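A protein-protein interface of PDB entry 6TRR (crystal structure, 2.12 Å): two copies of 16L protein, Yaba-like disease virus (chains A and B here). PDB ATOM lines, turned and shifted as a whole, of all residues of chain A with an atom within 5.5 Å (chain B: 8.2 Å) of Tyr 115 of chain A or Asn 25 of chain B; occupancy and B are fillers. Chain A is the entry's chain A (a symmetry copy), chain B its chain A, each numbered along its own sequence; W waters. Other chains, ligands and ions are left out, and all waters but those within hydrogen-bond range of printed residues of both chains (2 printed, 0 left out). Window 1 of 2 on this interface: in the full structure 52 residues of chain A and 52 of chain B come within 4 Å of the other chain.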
ATOM      1  N   LEU A  29     -16.431  30.462 -31.323  1.00  0.00           N
ATOM      2  CA  LEU A  29     -15.199  30.252 -32.076  1.00  0.00           C
ATOM      3  C   LEU A  29     -15.379  30.657 -33.532  1.00  0.00           C
ATOM      4  O   LEU A  29     -14.500  31.295 -34.121  1.00  0.00           O
ATOM      5  CB  LEU A  29     -14.761  28.791 -31.981  1.00  0.00           C
ATOM      6  CG  LEU A  29     -13.333  28.531 -32.468  1.00  0.00           C
ATOM      7  CD1 LEU A  29     -12.332  28.952 -31.397  1.00  0.00           C
ATOM      8  CD2 LEU A  29     -13.125  27.074 -32.881  1.00  0.00           C
ATOM      9  N   GLU A  32     -15.170  34.403 -33.672  1.00  0.00           N
ATOM     10  CA  GLU A  32     -13.805  34.882 -33.485  1.00  0.00           C
ATOM     11  C   GLU A  32     -12.970  34.669 -34.743  1.00  0.00           C
ATOM     12  O   GLU A  32     -12.135  35.511 -35.094  1.00  0.00           O
ATOM     13  CB  GLU A  32     -13.161  34.180 -32.288  1.00  0.00           C
ATOM     14  CG  GLU A  32     -11.963  34.923 -31.706  1.00  0.00           C
ATOM     15  CD  GLU A  32     -11.251  34.140 -30.610  1.00  0.00           C
ATOM     16  OE1 GLU A  32     -11.827  33.155 -30.102  1.00  0.00           O
ATOM     17  OE2 GLU A  32     -10.110  34.514 -30.258  1.00  0.00           O
ATOM     18  N   VAL A 110      -4.283  20.994 -23.021  1.00  0.00           N
ATOM     19  CA  VAL A 110      -5.712  21.069 -23.320  1.00  0.00           C
ATOM     20  C   VAL A 110      -6.195  19.767 -23.949  1.00  0.00           C
ATOM     21  O   VAL A 110      -7.327  19.329 -23.714  1.00  0.00           O
ATOM     22  CB  VAL A 110      -6.013  22.280 -24.223  1.00  0.00           C
ATOM     23  CG1 VAL A 110      -5.659  23.568 -23.514  1.00  0.00           C
ATOM     24  CG2 VAL A 110      -5.255  22.182 -25.533  1.00  0.00           C
ATOM     25  N   ASN A 113      -6.514  17.032 -20.880  1.00  0.00           N
ATOM     26  CA  ASN A 113      -7.574  17.195 -19.896  1.00  0.00           C
ATOM     27  C   ASN A 113      -8.839  17.820 -20.455  1.00  0.00           C
ATOM     28  O   ASN A 113      -9.894  17.708 -19.822  1.00  0.00           O
ATOM     29  CB  ASN A 113      -7.082  18.061 -18.728  1.00  0.00           C
ATOM     30  CG  ASN A 113      -5.846  17.494 -18.064  1.00  0.00           C
ATOM     31  OD1 ASN A 113      -5.706  16.278 -17.923  1.00  0.00           O
ATOM     32  ND2 ASN A 113      -4.936  18.371 -17.660  1.00  0.00           N
ATOM     33  N   GLY A 114      -8.767  18.465 -21.611  1.00  0.00           N
ATOM     34  CA  GLY A 114      -9.898  19.181 -22.154  1.00  0.00           C
ATOM     35  C   GLY A 114     -10.041  20.571 -21.564  1.00  0.00           C
ATOM     36  O   GLY A 114      -9.416  20.936 -20.565  1.00  0.00           O
ATOM     37  N   TYR A 115     -10.897  21.363 -22.205  1.00  0.00           N
ATOM     38  CA  TYR A 115     -11.119  22.743 -21.777  1.00  0.00           C
ATOM     39  C   TYR A 115     -12.409  23.240 -22.416  1.00  0.00           C
ATOM     40  O   TYR A 115     -12.471  23.420 -23.637  1.00  0.00           O
ATOM     41  CB  TYR A 115      -9.932  23.625 -22.150  1.00  0.00           C
ATOM     42  CG  TYR A 115     -10.140  25.103 -21.887  1.00  0.00           C
ATOM     43  CD1 TYR A 115     -10.445  25.568 -20.613  1.00  0.00           C
ATOM     44  CD2 TYR A 115     -10.014  26.033 -22.911  1.00  0.00           C
ATOM     45  CE1 TYR A 115     -10.632  26.920 -20.370  1.00  0.00           C
ATOM     46  CE2 TYR A 115     -10.198  27.385 -22.678  1.00  0.00           C
ATOM     47  CZ  TYR A 115     -10.506  27.823 -21.405  1.00  0.00           C
ATOM     48  OH  TYR A 115     -10.688  29.168 -21.170  1.00  0.00           O
ATOM     49  N   LYS A 116     -13.432  23.446 -21.589  1.00  0.00           N
ATOM     50  CA  LYS A 116     -14.713  23.980 -22.023  1.00  0.00           C
ATOM     51  C   LYS A 116     -14.909  25.437 -21.629  1.00  0.00           C
ATOM     52  O   LYS A 116     -15.990  25.988 -21.864  1.00  0.00           O
ATOM     53  CB  LYS A 116     -15.860  23.152 -21.430  1.00  0.00           C
ATOM     54  CG  LYS A 116     -15.778  21.664 -21.696  1.00  0.00           C
ATOM     55  CD  LYS A 116     -17.040  20.964 -21.212  1.00  0.00           C
ATOM     56  CE  LYS A 116     -17.074  19.508 -21.652  1.00  0.00           C
ATOM     57  NZ  LYS A 116     -18.335  18.828 -21.238  1.00  0.00           N
ATOM     58  N   GLY A 117     -13.903  26.072 -21.033  1.00  0.00           N
ATOM     59  CA  GLY A 117     -14.059  27.377 -20.443  1.00  0.00           C
ATOM     60  C   GLY A 117     -14.620  27.363 -19.040  1.00  0.00           C
ATOM     61  O   GLY A 117     -14.410  28.325 -18.292  1.00  0.00           O
ATOM     62  N   LYS A 118     -15.324  26.289 -18.662  1.00  0.00           N
ATOM     63  CA  LYS A 118     -15.839  26.168 -17.303  1.00  0.00           C
ATOM     64  C   LYS A 118     -14.726  26.302 -16.276  1.00  0.00           C
ATOM     65  O   LYS A 118     -14.957  26.803 -15.168  1.00  0.00           O
ATOM     66  CB  LYS A 118     -16.556  24.827 -17.128  1.00  0.00           C
ATOM     67  CG  LYS A 118     -17.507  24.461 -18.251  1.00  0.00           C
ATOM     68  CD  LYS A 118     -18.211  23.140 -17.970  1.00  0.00           C
ATOM     69  CE  LYS A 118     -19.227  22.848 -19.061  1.00  0.00           C
ATOM     70  NZ  LYS A 118     -20.026  21.613 -18.830  1.00  0.00           N
ATOM     71  N   ASN A 119     -13.517  25.868 -16.622  1.00  0.00           N
ATOM     72  CA  ASN A 119     -12.359  25.988 -15.740  1.00  0.00           C
ATOM     73  C   ASN A 119     -11.744  27.359 -15.993  1.00  0.00           C
ATOM     74  O   ASN A 119     -10.997  27.552 -16.956  1.00  0.00           O
ATOM     75  CB  ASN A 119     -11.368  24.857 -15.998  1.00  0.00           C
ATOM     76  CG  ASN A 119     -10.521  24.523 -14.781  1.00  0.00           C
ATOM     77  OD1 ASN A 119      -9.625  25.280 -14.408  1.00  0.00           O
ATOM     78  ND2 ASN A 119     -10.789  23.372 -14.170  1.00  0.00           N
ATOM     79  N   MET A 122      -7.833  27.895 -16.188  1.00  0.00           N
ATOM     80  CA  MET A 122      -7.253  27.651 -17.504  1.00  0.00           C
ATOM     81  C   MET A 122      -7.396  28.880 -18.396  1.00  0.00           C
ATOM     82  O   MET A 122      -6.502  29.189 -19.194  1.00  0.00           O
ATOM     83  CB  MET A 122      -7.913  26.432 -18.153  1.00  0.00           C
ATOM     84  CG  MET A 122      -7.295  25.096 -17.762  1.00  0.00           C
ATOM     85  SD  MET A 122      -5.555  24.956 -18.224  1.00  0.00           S
ATOM     86  CE  MET A 122      -5.648  25.078 -20.008  1.00  0.00           C
ATOM     87  N   SER A 123      -8.515  29.596 -18.272  1.00  0.00           N
ATOM     88  CA  SER A 123      -8.704  30.820 -19.043  1.00  0.00           C
ATOM     89  C   SER A 123      -7.628  31.849 -18.713  1.00  0.00           C
ATOM     90  O   SER A 123      -7.118  32.536 -19.606  1.00  0.00           O
ATOM     91  CB  SER A 123     -10.093  31.394 -18.770  1.00  0.00           C
ATOM     92  OG  SER A 123     -11.059  30.359 -18.651  1.00  0.00           O
ATOM     93  N   ILE A 126      -4.225  30.738 -20.300  1.00  0.00           N
ATOM     94  CA  ILE A 126      -4.166  31.033 -21.729  1.00  0.00           C
ATOM     95  C   ILE A 126      -3.936  32.525 -21.960  1.00  0.00           C
ATOM     96  O   ILE A 126      -3.047  32.921 -22.722  1.00  0.00           O
ATOM     97  CB  ILE A 126      -5.448  30.538 -22.423  1.00  0.00           C
ATOM     98  CG1 ILE A 126      -5.545  29.012 -22.314  1.00  0.00           C
ATOM     99  CG2 ILE A 126      -5.471  30.964 -23.892  1.00  0.00           C
ATOM    100  CD1 ILE A 126      -6.861  28.433 -22.782  1.00  0.00           C
ATOM    101  N   ASN B  18      -4.123  37.674 -29.905  1.00  0.00           N
ATOM    102  CA  ASN B  18      -5.433  37.200 -30.341  1.00  0.00           C
ATOM    103  C   ASN B  18      -5.317  35.886 -31.098  1.00  0.00           C
ATOM    104  O   ASN B  18      -6.144  34.983 -30.919  1.00  0.00           O
ATOM    105  CB  ASN B  18      -6.112  38.257 -31.210  1.00  0.00           C
ATOM    106  CG  ASN B  18      -6.518  39.483 -30.421  1.00  0.00           C
ATOM    107  OD1 ASN B  18      -6.780  39.405 -29.219  1.00  0.00           O
ATOM    108  ND2 ASN B  18      -6.570  40.627 -31.093  1.00  0.00           N
ATOM    109  N   VAL B  19      -4.299  35.757 -31.948  1.00  0.00           N
ATOM    110  CA  VAL B  19      -4.120  34.519 -32.700  1.00  0.00           C
ATOM    111  C   VAL B  19      -3.848  33.359 -31.749  1.00  0.00           C
ATOM    112  O   VAL B  19      -4.425  32.275 -31.891  1.00  0.00           O
ATOM    113  CB  VAL B  19      -3.004  34.694 -33.749  1.00  0.00           C
ATOM    114  CG1 VAL B  19      -2.510  33.346 -34.269  1.00  0.00           C
ATOM    115  CG2 VAL B  19      -3.518  35.539 -34.908  1.00  0.00           C
ATOM    116  N   ILE B  20      -2.985  33.572 -30.753  1.00  0.00           N
ATOM    117  CA  ILE B  20      -2.655  32.502 -29.814  1.00  0.00           C
ATOM    118  C   ILE B  20      -3.885  32.098 -29.008  1.00  0.00           C
ATOM    119  O   ILE B  20      -4.140  30.907 -28.796  1.00  0.00           O
ATOM    120  CB  ILE B  20      -1.493  32.934 -28.900  1.00  0.00           C
ATOM    121  CG1 ILE B  20      -0.216  33.104 -29.723  1.00  0.00           C
ATOM    122  CG2 ILE B  20      -1.278  31.916 -27.775  1.00  0.00           C
ATOM    123  CD1 ILE B  20       0.900  33.783 -28.987  1.00  0.00           C
ATOM    124  N   VAL B  21      -4.656  33.077 -28.532  1.00  0.00           N
ATOM    125  CA  VAL B  21      -5.868  32.765 -27.777  1.00  0.00           C
ATOM    126  C   VAL B  21      -6.820  31.939 -28.630  1.00  0.00           C
ATOM    127  O   VAL B  21      -7.388  30.942 -28.170  1.00  0.00           O
ATOM    128  CB  VAL B  21      -6.539  34.056 -27.274  1.00  0.00           C
ATOM    129  CG1 VAL B  21      -7.930  33.757 -26.713  1.00  0.00           C
ATOM    130  CG2 VAL B  21      -5.681  34.716 -26.211  1.00  0.00           C
ATOM    131  N   PHE B  22      -7.010  32.342 -29.887  1.00  0.00           N
ATOM    132  CA  PHE B  22      -7.896  31.592 -30.771  1.00  0.00           C
ATOM    133  C   PHE B  22      -7.357  30.190 -31.031  1.00  0.00           C
ATOM    134  O   PHE B  22      -8.097  29.202 -30.951  1.00  0.00           O
ATOM    135  CB  PHE B  22      -8.082  32.338 -32.088  1.00  0.00           C
ATOM    136  CG  PHE B  22      -8.836  31.548 -33.113  1.00  0.00           C
ATOM    137  CD1 PHE B  22     -10.220  31.537 -33.113  1.00  0.00           C
ATOM    138  CD2 PHE B  22      -8.163  30.798 -34.062  1.00  0.00           C
ATOM    139  CE1 PHE B  22     -10.916  30.804 -34.049  1.00  0.00           C
ATOM    140  CE2 PHE B  22      -8.856  30.062 -34.999  1.00  0.00           C
ATOM    141  CZ  PHE B  22     -10.235  30.065 -34.993  1.00  0.00           C
ATOM    142  N   TYR B  23      -6.066  30.088 -31.358  1.00  0.00           N
ATOM    143  CA  TYR B  23      -5.474  28.789 -31.670  1.00  0.00           C
ATOM    144  C   TYR B  23      -5.686  27.801 -30.531  1.00  0.00           C
ATOM    145  O   TYR B  23      -6.113  26.663 -30.752  1.00  0.00           O
ATOM    146  CB  TYR B  23      -3.983  28.956 -31.965  1.00  0.00           C
ATOM    147  CG  TYR B  23      -3.258  27.655 -32.239  1.00  0.00           C
ATOM    148  CD1 TYR B  23      -3.471  26.955 -33.420  1.00  0.00           C
ATOM    149  CD2 TYR B  23      -2.353  27.132 -31.323  1.00  0.00           C
ATOM    150  CE1 TYR B  23      -2.809  25.771 -33.678  1.00  0.00           C
ATOM    151  CE2 TYR B  23      -1.684  25.946 -31.573  1.00  0.00           C
ATOM    152  CZ  TYR B  23      -1.916  25.271 -32.753  1.00  0.00           C
ATOM    153  OH  TYR B  23      -1.256  24.090 -33.008  1.00  0.00           O
ATOM    154  N   ILE B  24      -5.391  28.220 -29.301  1.00  0.00           N
ATOM    155  CA  ILE B  24      -5.532  27.314 -28.167  1.00  0.00           C
ATOM    156  C   ILE B  24      -7.001  27.002 -27.914  1.00  0.00           C
ATOM    157  O   ILE B  24      -7.365  25.847 -27.662  1.00  0.00           O
ATOM    158  CB  ILE B  24      -4.846  27.906 -26.924  1.00  0.00           C
ATOM    159  CG1 ILE B  24      -3.333  27.956 -27.146  1.00  0.00           C
ATOM    160  CG2 ILE B  24      -5.170  27.073 -25.687  1.00  0.00           C
ATOM    161  CD1 ILE B  24      -2.570  28.709 -26.080  1.00  0.00           C
ATOM    162  N   ASN B  25      -7.869  28.015 -27.980  1.00  0.00           N
ATOM    163  CA  ASN B  25      -9.302  27.759 -27.839  1.00  0.00           C
ATOM    164  C   ASN B  25      -9.783  26.764 -28.889  1.00  0.00           C
ATOM    165  O   ASN B  25     -10.592  25.877 -28.590  1.00  0.00           O
ATOM    166  CB  ASN B  25     -10.096  29.065 -27.944  1.00  0.00           C
ATOM    167  CG  ASN B  25      -9.998  29.921 -26.689  1.00  0.00           C
ATOM    168  OD1 ASN B  25      -9.585  29.451 -25.629  1.00  0.00           O
ATOM    169  ND2 ASN B  25     -10.396  31.185 -26.803  1.00  0.00           N
ATOM    170  N   GLU B  26      -9.294  26.892 -30.125  1.00  0.00           N
ATOM    171  CA  GLU B  26      -9.667  25.952 -31.178  1.00  0.00           C
ATOM    172  C   GLU B  26      -9.231  24.535 -30.823  1.00  0.00           C
ATOM    173  O   GLU B  26     -10.001  23.579 -30.971  1.00  0.00           O
ATOM    174  CB  GLU B  26      -9.052  26.389 -32.509  1.00  0.00           C
ATOM    175  CG  GLU B  26      -9.518  25.594 -33.718  1.00  0.00           C
ATOM    176  CD  GLU B  26      -8.809  26.010 -34.997  1.00  0.00           C
ATOM    177  OE1 GLU B  26      -7.572  26.194 -34.965  1.00  0.00           O
ATOM    178  OE2 GLU B  26      -9.487  26.158 -36.034  1.00  0.00           O
ATOM    179  N   LYS B  27      -7.992  24.380 -30.348  1.00  0.00           N
ATOM    180  CA  LYS B  27      -7.519  23.063 -29.936  1.00  0.00           C
ATOM    181  C   LYS B  27      -8.390  22.483 -28.831  1.00  0.00           C
ATOM    182  O   LYS B  27      -8.607  21.267 -28.782  1.00  0.00           O
ATOM    183  CB  LYS B  27      -6.062  23.151 -29.476  1.00  0.00           C
ATOM    184  CG  LYS B  27      -5.082  23.458 -30.597  1.00  0.00           C
ATOM    185  CD  LYS B  27      -4.715  22.204 -31.375  1.00  0.00           C
ATOM    186  CE  LYS B  27      -4.275  22.537 -32.790  1.00  0.00           C
ATOM    187  NZ  LYS B  27      -3.380  21.496 -33.367  1.00  0.00           N
ATOM    188  N   ALA B  28      -8.901  23.336 -27.941  1.00  0.00           N
ATOM    189  CA  ALA B  28      -9.758  22.864 -26.858  1.00  0.00           C
ATOM    190  C   ALA B  28     -11.116  22.420 -27.384  1.00  0.00           C
ATOM    191  O   ALA B  28     -11.630  21.365 -26.992  1.00  0.00           O
ATOM    192  CB  ALA B  28      -9.927  23.964 -25.812  1.00  0.00           C
ATOM    193  N   LEU B  29     -11.724  23.224 -28.260  1.00  0.00           N
ATOM    194  CA  LEU B  29     -13.004  22.837 -28.844  1.00  0.00           C
ATOM    195  C   LEU B  29     -12.900  21.479 -29.524  1.00  0.00           C
ATOM    196  O   LEU B  29     -13.795  20.638 -29.391  1.00  0.00           O
ATOM    197  CB  LEU B  29     -13.474  23.895 -29.842  1.00  0.00           C
ATOM    198  CG  LEU B  29     -14.935  23.745 -30.275  1.00  0.00           C
ATOM    199  CD1 LEU B  29     -15.858  24.287 -29.189  1.00  0.00           C
ATOM    200  CD2 LEU B  29     -15.205  24.417 -31.620  1.00  0.00           C
ATOM    201  N   ILE B  30     -11.812  21.250 -30.262  1.00  0.00           N
ATOM    202  CA  ILE B  30     -11.607  19.957 -30.907  1.00  0.00           C
ATOM    203  C   ILE B  30     -11.623  18.842 -29.868  1.00  0.00           C
ATOM    204  O   ILE B  30     -12.272  17.806 -30.057  1.00  0.00           O
ATOM    205  CB  ILE B  30     -10.294  19.974 -31.716  1.00  0.00           C
ATOM    206  CG1 ILE B  30     -10.410  20.971 -32.874  1.00  0.00           C
ATOM    207  CG2 ILE B  30      -9.959  18.579 -32.247  1.00  0.00           C
ATOM    208  CD1 ILE B  30      -9.108  21.282 -33.557  1.00  0.00           C
ATOM    209  N   GLU B  31     -10.922  19.041 -28.749  1.00  0.00           N
ATOM    210  CA  GLU B  31     -10.900  18.024 -27.702  1.00  0.00           C
ATOM    211  C   GLU B  31     -12.290  17.797 -27.121  1.00  0.00           C
ATOM    212  O   GLU B  31     -12.711  16.650 -26.931  1.00  0.00           O
ATOM    213  CB  GLU B  31      -9.921  18.427 -26.601  1.00  0.00           C
ATOM    214  CG  GLU B  31      -9.805  17.414 -25.472  1.00  0.00           C
ATOM    215  CD  GLU B  31      -9.458  16.022 -25.970  1.00  0.00           C
ATOM    216  OE1 GLU B  31      -9.903  15.038 -25.343  1.00  0.00           O
ATOM    217  OE2 GLU B  31      -8.745  15.914 -26.990  1.00  0.00           O
ATOM    218  N   GLU B  32     -13.016  18.877 -26.821  1.00  0.00           N
ATOM    219  CA  GLU B  32     -14.355  18.732 -26.258  1.00  0.00           C
ATOM    220  C   GLU B  32     -15.269  17.961 -27.204  1.00  0.00           C
ATOM    221  O   GLU B  32     -16.102  17.161 -26.762  1.00  0.00           O
ATOM    222  CB  GLU B  32     -14.946  20.109 -25.945  1.00  0.00           C
ATOM    223  CG  GLU B  32     -16.086  20.077 -24.933  1.00  0.00           C
ATOM    224  CD  GLU B  32     -16.753  21.434 -24.743  1.00  0.00           C
ATOM    225  OE1 GLU B  32     -16.173  22.454 -25.171  1.00  0.00           O
ATOM    226  OE2 GLU B  32     -17.859  21.477 -24.162  1.00  0.00           O
ATOM    227  N   LYS B  33     -15.125  18.188 -28.512  1.00  0.00           N
ATOM    228  CA  LYS B  33     -15.926  17.458 -29.491  1.00  0.00           C
ATOM    229  C   LYS B  33     -15.630  15.965 -29.434  1.00  0.00           C
ATOM    230  O   LYS B  33     -16.549  15.139 -29.392  1.00  0.00           O
ATOM    231  CB  LYS B  33     -15.659  18.013 -30.892  1.00  0.00           C
ATOM    232  CG  LYS B  33     -16.340  17.262 -32.036  1.00  0.00           C
ATOM    233  CD  LYS B  33     -17.849  17.422 -32.018  1.00  0.00           C
ATOM    234  CE  LYS B  33     -18.473  16.806 -33.262  1.00  0.00           C
ATOM    235  NZ  LYS B  33     -19.953  16.959 -33.303  1.00  0.00           N
ATOM    236  N   MET B  35     -14.644  14.241 -27.011  1.00  0.00           N
ATOM    237  CA  MET B  35     -15.142  13.678 -25.764  1.00  0.00           C
ATOM    238  C   MET B  35     -16.660  13.577 -25.720  1.00  0.00           C
ATOM    239  O   MET B  35     -17.196  12.989 -24.775  1.00  0.00           O
ATOM    240  CB  MET B  35     -14.650  14.517 -24.581  1.00  0.00           C
ATOM    241  CG  MET B  35     -13.130  14.566 -24.432  1.00  0.00           C
ATOM    242  SD  MET B  35     -12.367  12.948 -24.173  1.00  0.00           S
ATOM    243  CE  MET B  35     -11.931  12.472 -25.849  1.00  0.00           C
ATOM    244  N   TYR B 115     -16.945  36.230 -28.624  1.00  0.00           N
ATOM    245  CA  TYR B 115     -16.661  35.621 -27.326  1.00  0.00           C
ATOM    246  C   TYR B 115     -15.399  34.778 -27.459  1.00  0.00           C
ATOM    247  O   TYR B 115     -15.404  33.749 -28.142  1.00  0.00           O
ATOM    248  CB  TYR B 115     -17.845  34.785 -26.848  1.00  0.00           C
ATOM    249  CG  TYR B 115     -17.583  33.987 -25.586  1.00  0.00           C
ATOM    250  CD1 TYR B 115     -17.190  34.615 -24.410  1.00  0.00           C
ATOM    251  CD2 TYR B 115     -17.744  32.608 -25.569  1.00  0.00           C
ATOM    252  CE1 TYR B 115     -16.953  33.888 -23.254  1.00  0.00           C
ATOM    253  CE2 TYR B 115     -17.511  31.873 -24.420  1.00  0.00           C
ATOM    254  CZ  TYR B 115     -17.115  32.518 -23.264  1.00  0.00           C
ATOM    255  OH  TYR B 115     -16.884  31.790 -22.119  1.00  0.00           O
ATOM    256  N   LYS B 116     -14.324  35.229 -26.816  1.00  0.00           N
ATOM    257  CA  LYS B 116     -13.056  34.515 -26.784  1.00  0.00           C
ATOM    258  C   LYS B 116     -12.798  33.830 -25.450  1.00  0.00           C
ATOM    259  O   LYS B 116     -11.719  33.258 -25.262  1.00  0.00           O
ATOM    260  CB  LYS B 116     -11.899  35.478 -27.073  1.00  0.00           C
ATOM    261  CG  LYS B 116     -12.036  36.278 -28.352  1.00  0.00           C
ATOM    262  CD  LYS B 116     -10.766  37.072 -28.625  1.00  0.00           C
ATOM    263  CE  LYS B 116     -10.797  37.716 -30.003  1.00  0.00           C
ATOM    264  NZ  LYS B 116      -9.533  38.445 -30.308  1.00  0.00           N
ATOM    265  N   GLY B 117     -13.751  33.875 -24.521  1.00  0.00           N
ATOM    266  CA  GLY B 117     -13.525  33.437 -23.167  1.00  0.00           C
ATOM    267  C   GLY B 117     -12.881  34.476 -22.277  1.00  0.00           C
ATOM    268  O   GLY B 117     -13.021  34.395 -21.051  1.00  0.00           O
ATOM    269  N   LYS B 118     -12.186  35.455 -22.865  1.00  0.00           N
ATOM    270  CA  LYS B 118     -11.594  36.533 -22.081  1.00  0.00           C
ATOM    271  C   LYS B 118     -12.639  37.237 -21.230  1.00  0.00           C
ATOM    272  O   LYS B 118     -12.329  37.719 -20.134  1.00  0.00           O
ATOM    273  CB  LYS B 118     -10.904  37.539 -23.003  1.00  0.00           C
ATOM    274  CG  LYS B 118     -10.032  36.924 -24.081  1.00  0.00           C
ATOM    275  CD  LYS B 118      -9.346  37.997 -24.917  1.00  0.00           C
ATOM    276  CE  LYS B 118      -8.405  37.354 -25.921  1.00  0.00           C
ATOM    277  NZ  LYS B 118      -7.627  38.330 -26.734  1.00  0.00           N
ATOM    278  N   ILE B 120     -15.167  36.810 -18.812  1.00  0.00           N
ATOM    279  CA  ILE B 120     -15.567  35.770 -17.866  1.00  0.00           C
ATOM    280  C   ILE B 120     -17.062  35.865 -17.570  1.00  0.00           C
ATOM    281  O   ILE B 120     -17.717  34.827 -17.409  1.00  0.00           O
ATOM    282  CB  ILE B 120     -14.729  35.853 -16.578  1.00  0.00           C
ATOM    283  CG1 ILE B 120     -13.285  35.447 -16.883  1.00  0.00           C
ATOM    284  CG2 ILE B 120     -15.305  34.960 -15.483  1.00  0.00           C
ATOM    285  CD1 ILE B 120     -12.302  35.786 -15.789  1.00  0.00           C
ATOM    286  N   SER B 123     -18.869  33.716 -19.741  1.00  0.00           N
ATOM    287  CA  SER B 123     -18.693  32.321 -19.355  1.00  0.00           C
ATOM    288  C   SER B 123     -19.720  31.907 -18.307  1.00  0.00           C
ATOM    289  O   SER B 123     -20.264  30.797 -18.360  1.00  0.00           O
ATOM    290  CB  SER B 123     -17.275  32.103 -18.829  1.00  0.00           C
ATOM    291  OG  SER B 123     -16.333  32.857 -19.577  1.00  0.00           O
HETATM  292  O   HOH W   1     -18.034  28.717 -21.652  1.00  0.00           O
HETATM  293  O   HOH W   2      -9.594  31.538 -23.213  1.00  0.00           O
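Of the printed residues of chain B, Leu 29 of chain A touches Phe 22, Glu 26 and Leu 29. Gly 114 of chain A touches just one residue of chain B: Glu 31. Tyr 115 of chain A touches just these residues of chain B: Asn 25 (3.7 Å) and Ala 28 (3.4 Å). Of the printed residues of chain A, Ile 24 of chain B touches Ile 126 (3.6 Å). Of chain A, only Tyr 115 (3.7 Å) comes within 4 Å of Asn 25 of chain B. Printed residues of chain A within 4 Å of Glu 32 of chain B: Lys 116. Of the printed residues of chain A, Lys 116 of chain B touches Glu 32 (3.1 Å). The nearest residue of chain B that does not touch Tyr 115 of chain A is Glu 32 of chain B (4.1 Å). The nearest printed residue of chain B that does not touch Lys 116 of chain A is Ala 28 of chain B (5.5 Å).
Leu 29 of chain B touches its own counterpart, Leu 29 of chain A. Glu 32 of chain A touches Lys 116 of chain B, and with the chains exchanged Lys 116 of chain A touches Glu 32 of chain B. Of the 11 pairs that touch across the chains among the printed residues, 3 have their exchanged pair printed and touching as well.
OD1 of Asn 18 of chain B lies within hydrogen-bond range of NZ of Lys 116 of chain B, at 3.1 Å. ND2 of Asn 25 of chain B sits close to O of Val 21 of chain B, at 3.3 Å. ND2 of Asn 25 of chain B is in hydrogen-bond range of O of Lys 116 of chain B. The side-chain hydroxyl (OH) of Tyr 115 of chain A sits at hydrogen-bond distance from the side-chain hydroxyl (OG) of Ser 123 of chain A (2.8 Å).
Water W2 lies within hydrogen-bond range of OD1 of Asn 25 of chain B, OH of Tyr 115 of chain A and O of Lys 116 of chain B. Water W1 bridges OH of Tyr 115 of chain B (3.3 Å) and O of Lys 116 of chain A (3.4 Å).
OE2 of Glu 32 of chain B is in salt-bridge range of NZ of Lys 116 of chain A. NZ of Lys 116 of chain B lies within salt-bridge range of OE2 of Glu 32 of chain A, 3.97 Å away.
Of the 13 printed residues of chain A, 7 touch a printed residue of chain B. Hydrophobic or aromatic side chains of chain A within 4 Å of the printed part of chain B: Leu 29, Tyr 115 and Ile 126. Among the printed residues, 11 pairs touch across the chains. Among the printed residues, Asp or Glu carboxylates within 4 Å of a Lys or Arg side-chain nitrogen of the other chain: Glu 32 of chain A with Lys 116 of chain B (3.97 Å) and Lys 116 of chain A with Glu 32 of chain B (3.97 Å).
Among the printed residues, pairs that only touch across the chains: Tyr 115 of chain A with Ala 28 of chain B (3.4 Å), Glu 32 of chain A with Phe 22 of chain B (3.5 Å), Leu 29 of chain A with Phe 22 of chain B (3.5 Å), Val 110 of chain A with Glu 31 of chain B (3.6 Å), Leu 29 of chain A with Leu 29 of chain B (3.6 Å), Ile 126 of chain A with Ile 24 of chain B (3.6 Å), Tyr 115 of chain A with Asn 25 of chain B (3.7 Å), Gly 114 of chain A with Glu 31 of chain B (3.8 Å) and Leu 29 of chain A with Glu 26 of chain B (3.9 Å).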
